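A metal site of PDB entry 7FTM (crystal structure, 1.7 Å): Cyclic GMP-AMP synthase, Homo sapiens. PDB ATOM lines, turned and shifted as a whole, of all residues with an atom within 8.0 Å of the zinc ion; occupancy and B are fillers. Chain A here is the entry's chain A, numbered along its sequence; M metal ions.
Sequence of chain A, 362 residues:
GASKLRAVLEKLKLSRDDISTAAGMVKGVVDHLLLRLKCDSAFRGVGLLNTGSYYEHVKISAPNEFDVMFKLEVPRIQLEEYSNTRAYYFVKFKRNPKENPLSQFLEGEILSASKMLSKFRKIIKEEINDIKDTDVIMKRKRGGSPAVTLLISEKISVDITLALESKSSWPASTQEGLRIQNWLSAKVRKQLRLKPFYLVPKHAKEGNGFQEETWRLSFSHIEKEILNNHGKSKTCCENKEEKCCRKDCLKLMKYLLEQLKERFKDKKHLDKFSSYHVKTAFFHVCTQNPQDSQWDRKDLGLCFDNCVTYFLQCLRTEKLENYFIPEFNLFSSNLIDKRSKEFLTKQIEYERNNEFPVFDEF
O of His 230 sits at hydrogen-bond distance from NE of Arg 246.
A ring nitrogen (ND1) of His 230 lies within hydrogen-bond range of the backbone carbonyl oxygen (O) of Leu 227 (3.0 Å).
The guanidinium group (NH2) of Arg 246 lies close to the side-chain sulfur (SG) of Cys 244, 3.4 Å away.
NZ of Lys 243 sits at hydrogen-bond distance from O of Cys 237, 3.1 Å away.
The guanidinium group (NH2) of Arg 246 sits close to the side-chain sulfur (SG) of Cys 236 (3.7 Å).
N of Cys 237 lies within hydrogen-bond range of O of Glu 242.
Of the 20 residues printed, 4 come within 4 Å of the zinc ion.
The nearest printed residue that does not touch the zinc ion is Arg 246 (4.3 Å).
The zinc ion is bound by NE2 of His 230 (2.0 Å), SG of Cys 237 (2.3 Å), SG of Cys 236 (2.3 Å) and SG of Cys 244 (2.4 Å).
The zinc ion has four donor atoms within binding distance.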
ATOM      1  N   LEU A 227       3.463 -20.090 -16.669  1.00  0.00           N
ATOM      2  CA  LEU A 227       4.233 -20.216 -15.433  1.00  0.00           C
ATOM      3  C   LEU A 227       3.748 -21.404 -14.607  1.00  0.00           C
ATOM      4  O   LEU A 227       4.541 -22.104 -13.965  1.00  0.00           O
ATOM      5  CB  LEU A 227       4.112 -18.941 -14.603  1.00  0.00           C
ATOM      6  CG  LEU A 227       5.291 -17.993 -14.764  1.00  0.00           C
ATOM      7  CD1 LEU A 227       4.960 -16.654 -14.130  1.00  0.00           C
ATOM      8  CD2 LEU A 227       6.491 -18.663 -14.073  1.00  0.00           C
ATOM      9  N   ASN A 228       2.443 -21.643 -14.637  1.00  0.00           N
ATOM     10  CA  ASN A 228       1.853 -22.703 -13.852  1.00  0.00           C
ATOM     11  C   ASN A 228       1.949 -24.061 -14.546  1.00  0.00           C
ATOM     12  O   ASN A 228       2.053 -25.088 -13.871  1.00  0.00           O
ATOM     13  CB  ASN A 228       0.408 -22.358 -13.530  1.00  0.00           C
ATOM     14  CG  ASN A 228       0.304 -21.410 -12.343  1.00  0.00           C
ATOM     15  OD1 ASN A 228       1.318 -21.041 -11.733  1.00  0.00           O
ATOM     16  ND2 ASN A 228      -0.921 -21.003 -12.008  1.00  0.00           N
ATOM     17  N   ASN A 229       1.932 -24.098 -15.879  1.00  0.00           N
ATOM     18  CA  ASN A 229       2.021 -25.330 -16.648  1.00  0.00           C
ATOM     19  C   ASN A 229       3.309 -25.249 -17.474  1.00  0.00           C
ATOM     20  O   ASN A 229       3.297 -24.980 -18.681  1.00  0.00           O
ATOM     21  CB  ASN A 229       0.729 -25.485 -17.503  1.00  0.00           C
ATOM     22  CG  ASN A 229       0.600 -26.848 -18.134  1.00  0.00           C
ATOM     23  OD1 ASN A 229       1.457 -27.719 -17.975  1.00  0.00           O
ATOM     24  ND2 ASN A 229      -0.503 -27.057 -18.838  1.00  0.00           N
ATOM     25  N   HIS A 230       4.436 -25.430 -16.804  1.00  0.00           N
ATOM     26  CA  HIS A 230       5.687 -24.826 -17.261  1.00  0.00           C
ATOM     27  C   HIS A 230       6.704 -25.834 -17.759  1.00  0.00           C
ATOM     28  O   HIS A 230       7.834 -25.440 -18.086  1.00  0.00           O
ATOM     29  CB  HIS A 230       6.329 -24.022 -16.133  1.00  0.00           C
ATOM     30  CG  HIS A 230       6.616 -24.880 -14.921  1.00  0.00           C
ATOM     31  ND1 HIS A 230       6.036 -24.637 -13.703  1.00  0.00           N
ATOM     32  CD2 HIS A 230       7.390 -25.977 -14.775  1.00  0.00           C
ATOM     33  CE1 HIS A 230       6.446 -25.564 -12.830  1.00  0.00           C
ATOM     34  NE2 HIS A 230       7.263 -26.394 -13.469  1.00  0.00           N
ATOM     35  N   GLY A 231       6.391 -27.135 -17.706  1.00  0.00           N
ATOM     36  CA  GLY A 231       7.368 -28.152 -17.999  1.00  0.00           C
ATOM     37  C   GLY A 231       7.246 -28.653 -19.420  1.00  0.00           C
ATOM     38  O   GLY A 231       6.189 -28.543 -20.057  1.00  0.00           O
ATOM     39  N   LYS A 232       8.343 -29.210 -19.941  1.00  0.00           N
ATOM     40  CA  LYS A 232       8.200 -30.007 -21.152  1.00  0.00           C
ATOM     41  C   LYS A 232       7.359 -31.242 -20.870  1.00  0.00           C
ATOM     42  O   LYS A 232       6.451 -31.575 -21.634  1.00  0.00           O
ATOM     43  CB  LYS A 232       9.554 -30.408 -21.748  1.00  0.00           C
ATOM     44  CG  LYS A 232       9.353 -31.412 -22.916  1.00  0.00           C
ATOM     45  CD  LYS A 232      10.622 -31.695 -23.710  1.00  0.00           C
ATOM     46  CE  LYS A 232      11.145 -30.429 -24.362  1.00  0.00           C
ATOM     47  NZ  LYS A 232      10.161 -29.846 -25.380  1.00  0.00           N
ATOM     48  N   SER A 233       7.632 -31.910 -19.744  1.00  0.00           N
ATOM     49  CA  SER A 233       6.758 -32.968 -19.279  1.00  0.00           C
ATOM     50  C   SER A 233       5.439 -32.377 -18.783  1.00  0.00           C
ATOM     51  O   SER A 233       5.452 -31.451 -17.952  1.00  0.00           O
ATOM     52  CB  SER A 233       7.401 -33.714 -18.118  1.00  0.00           C
ATOM     53  OG  SER A 233       6.459 -34.670 -17.665  1.00  0.00           O
ATOM     54  N   THR A 235       3.668 -33.741 -16.579  1.00  0.00           N
ATOM     55  CA  THR A 235       3.662 -33.971 -15.130  1.00  0.00           C
ATOM     56  C   THR A 235       4.825 -33.303 -14.366  1.00  0.00           C
ATOM     57  O   THR A 235       5.090 -33.694 -13.210  1.00  0.00           O
ATOM     58  CB  THR A 235       3.618 -35.484 -14.842  1.00  0.00           C
ATOM     59  OG1 THR A 235       4.580 -36.191 -15.635  1.00  0.00           O
ATOM     60  CG2 THR A 235       2.223 -36.057 -15.155  1.00  0.00           C
ATOM     61  N   CYS A 236       5.505 -32.295 -14.966  1.00  0.00           N
ATOM     62  CA  CYS A 236       6.512 -31.506 -14.249  1.00  0.00           C
ATOM     63  C   CYS A 236       5.907 -30.949 -12.971  1.00  0.00           C
ATOM     64  O   CYS A 236       4.780 -30.436 -12.984  1.00  0.00           O
ATOM     65  CB  CYS A 236       7.023 -30.318 -15.097  1.00  0.00           C
ATOM     66  SG  CYS A 236       8.591 -29.582 -14.551  1.00  0.00           S
ATOM     67  N   CYS A 237       6.610 -31.165 -11.859  1.00  0.00           N
ATOM     68  CA  CYS A 237       6.182 -30.727 -10.524  1.00  0.00           C
ATOM     69  C   CYS A 237       4.891 -31.385 -10.015  1.00  0.00           C
ATOM     70  O   CYS A 237       4.366 -30.977  -8.963  1.00  0.00           O
ATOM     71  CB  CYS A 237       6.109 -29.188 -10.510  1.00  0.00           C
ATOM     72  SG  CYS A 237       7.821 -28.413 -10.544  1.00  0.00           S
ATOM     73  N   GLU A 238       4.393 -32.457 -10.640  1.00  0.00           N
ATOM     74  CA  GLU A 238       3.241 -33.171 -10.105  1.00  0.00           C
ATOM     75  C   GLU A 238       3.611 -34.436  -9.336  1.00  0.00           C
ATOM     76  O   GLU A 238       2.718 -35.104  -8.795  1.00  0.00           O
ATOM     77  CB  GLU A 238       2.259 -33.557 -11.240  1.00  0.00           C
ATOM     78  CG  GLU A 238       1.541 -32.364 -11.866  1.00  0.00           C
ATOM     79  CD  GLU A 238       0.303 -32.774 -12.675  1.00  0.00           C
ATOM     80  OE1 GLU A 238       0.090 -33.997 -12.875  1.00  0.00           O
ATOM     81  OE2 GLU A 238      -0.458 -31.874 -13.091  1.00  0.00           O
ATOM     82  N   GLU A 242       9.797 -35.459 -10.530  1.00  0.00           N
ATOM     83  CA  GLU A 242       9.824 -34.407 -11.546  1.00  0.00           C
ATOM     84  C   GLU A 242       9.692 -33.039 -10.886  1.00  0.00           C
ATOM     85  O   GLU A 242       8.810 -32.253 -11.184  1.00  0.00           O
ATOM     86  CB  GLU A 242       8.722 -34.589 -12.578  1.00  0.00           C
ATOM     87  CG  GLU A 242       8.854 -35.885 -13.411  1.00  0.00           C
ATOM     88  CD  GLU A 242       7.772 -35.940 -14.467  1.00  0.00           C
ATOM     89  OE1 GLU A 242       7.860 -35.173 -15.439  1.00  0.00           O
ATOM     90  OE2 GLU A 242       6.822 -36.739 -14.313  1.00  0.00           O
ATOM     91  N   LYS A 243      10.636 -32.714 -10.015  1.00  0.00           N
ATOM     92  CA  LYS A 243      10.618 -31.442  -9.316  1.00  0.00           C
ATOM     93  C   LYS A 243      11.628 -30.511  -9.985  1.00  0.00           C
ATOM     94  O   LYS A 243      12.838 -30.734  -9.885  1.00  0.00           O
ATOM     95  CB  LYS A 243      10.942 -31.638  -7.838  1.00  0.00           C
ATOM     96  CG  LYS A 243       9.749 -32.161  -7.029  1.00  0.00           C
ATOM     97  CD  LYS A 243       8.573 -31.202  -7.208  1.00  0.00           C
ATOM     98  CE  LYS A 243       7.322 -31.567  -6.410  1.00  0.00           C
ATOM     99  NZ  LYS A 243       6.292 -30.471  -6.568  1.00  0.00           N
ATOM    100  N   CYS A 244      11.143 -29.477 -10.669  1.00  0.00           N
ATOM    101  CA  CYS A 244      12.075 -28.510 -11.242  1.00  0.00           C
ATOM    102  C   CYS A 244      12.142 -27.246 -10.383  1.00  0.00           C
ATOM    103  O   CYS A 244      11.367 -27.060  -9.457  1.00  0.00           O
ATOM    104  CB  CYS A 244      11.703 -28.144 -12.683  1.00  0.00           C
ATOM    105  SG  CYS A 244      10.335 -26.916 -12.874  1.00  0.00           S
ATOM    106  N   CYS A 245      13.082 -26.360 -10.727  1.00  0.00           N
ATOM    107  CA  CYS A 245      13.270 -25.136  -9.964  1.00  0.00           C
ATOM    108  C   CYS A 245      12.902 -23.898 -10.767  1.00  0.00           C
ATOM    109  O   CYS A 245      13.390 -22.815 -10.464  1.00  0.00           O
ATOM    110  CB  CYS A 245      14.709 -25.031  -9.458  1.00  0.00           C
ATOM    111  SG  CYS A 245      15.979 -24.888 -10.782  1.00  0.00           S
ATOM    112  N   ARG A 246      12.033 -24.037 -11.780  1.00  0.00           N
ATOM    113  CA  ARG A 246      11.706 -22.877 -12.620  1.00  0.00           C
ATOM    114  C   ARG A 246      11.045 -21.767 -11.799  1.00  0.00           C
ATOM    115  O   ARG A 246      11.481 -20.603 -11.872  1.00  0.00           O
ATOM    116  CB  ARG A 246      10.802 -23.300 -13.787  1.00  0.00           C
ATOM    117  CG  ARG A 246      11.519 -24.027 -14.925  1.00  0.00           C
ATOM    118  CD  ARG A 246      10.520 -24.206 -16.068  1.00  0.00           C
ATOM    119  NE  ARG A 246      11.047 -24.943 -17.227  1.00  0.00           N
ATOM    120  CZ  ARG A 246      11.005 -26.263 -17.325  1.00  0.00           C
ATOM    121  NH1 ARG A 246      11.406 -26.851 -18.469  1.00  0.00           N
ATOM    122  NH2 ARG A 246      10.584 -27.002 -16.288  1.00  0.00           N
ATOM    123  N   LYS A 247      10.008 -22.098 -11.042  1.00  0.00           N
ATOM    124  CA  LYS A 247       9.298 -21.083 -10.259  1.00  0.00           C
ATOM    125  C   LYS A 247      10.221 -20.446  -9.222  1.00  0.00           C
ATOM    126  O   LYS A 247      10.182 -19.227  -9.001  1.00  0.00           O
ATOM    127  CB  LYS A 247       8.059 -21.662  -9.579  1.00  0.00           C
ATOM    128  CG  LYS A 247       6.830 -21.812 -10.511  1.00  0.00           C
ATOM    129  CD  LYS A 247       5.593 -22.120  -9.671  1.00  0.00           C
ATOM    130  CE  LYS A 247       4.386 -22.434 -10.536  1.00  0.00           C
ATOM    131  NZ  LYS A 247       3.175 -22.655  -9.685  1.00  0.00           N
ATOM    132  N   ASP A 292      13.327 -30.209 -19.077  1.00  0.00           N
ATOM    133  CA  ASP A 292      13.158 -30.195 -17.624  1.00  0.00           C
ATOM    134  C   ASP A 292      14.459 -30.543 -16.900  1.00  0.00           C
ATOM    135  O   ASP A 292      14.703 -30.064 -15.794  1.00  0.00           O
ATOM    136  CB  ASP A 292      12.032 -31.163 -17.224  1.00  0.00           C
ATOM    137  CG  ASP A 292      10.656 -30.755 -17.785  1.00  0.00           C
ATOM    138  OD1 ASP A 292      10.443 -29.564 -18.078  1.00  0.00           O
ATOM    139  OD2 ASP A 292       9.787 -31.630 -17.957  1.00  0.00           O
ATOM    140  N   TRP A 295      16.544 -27.819 -15.447  1.00  0.00           N
ATOM    141  CA  TRP A 295      15.943 -27.100 -14.331  1.00  0.00           C
ATOM    142  C   TRP A 295      15.826 -28.008 -13.118  1.00  0.00           C
ATOM    143  O   TRP A 295      14.929 -27.837 -12.278  1.00  0.00           O
ATOM    144  CB  TRP A 295      14.582 -26.539 -14.724  1.00  0.00           C
ATOM    145  CG  TRP A 295      14.670 -25.510 -15.830  1.00  0.00           C
ATOM    146  CD1 TRP A 295      14.567 -25.741 -17.198  1.00  0.00           C
ATOM    147  CD2 TRP A 295      14.944 -24.102 -15.697  1.00  0.00           C
ATOM    148  NE1 TRP A 295      14.750 -24.570 -17.890  1.00  0.00           N
ATOM    149  CE2 TRP A 295      14.962 -23.548 -16.994  1.00  0.00           C
ATOM    150  CE3 TRP A 295      15.153 -23.262 -14.589  1.00  0.00           C
ATOM    151  CZ2 TRP A 295      15.168 -22.182 -17.226  1.00  0.00           C
ATOM    152  CZ3 TRP A 295      15.365 -21.888 -14.823  1.00  0.00           C
ATOM    153  CH2 TRP A 295      15.369 -21.378 -16.126  1.00  0.00           C
ATOM    154  N   ARG A 297      15.869 -29.491  -9.653  1.00  0.00           N
ATOM    155  CA  ARG A 297      15.895 -28.951  -8.295  1.00  0.00           C
ATOM    156  C   ARG A 297      17.295 -28.887  -7.699  1.00  0.00           C
ATOM    157  O   ARG A 297      17.678 -27.888  -7.066  1.00  0.00           O
ATOM    158  CB  ARG A 297      14.993 -29.839  -7.423  1.00  0.00           C
ATOM    159  CG  ARG A 297      14.583 -29.257  -6.107  1.00  0.00           C
ATOM    160  CD  ARG A 297      13.457 -28.279  -6.314  1.00  0.00           C
ATOM    161  NE  ARG A 297      12.530 -28.297  -5.194  1.00  0.00           N
ATOM    162  CZ  ARG A 297      11.520 -27.444  -5.066  1.00  0.00           C
ATOM    163  NH1 ARG A 297      10.714 -27.516  -4.016  1.00  0.00           N
ATOM    164  NH2 ARG A 297      11.327 -26.499  -5.983  1.00  0.00           N
HETATM  165 ZN    ZN M   1       8.248 -28.059 -12.804  1.00  0.00          ZN
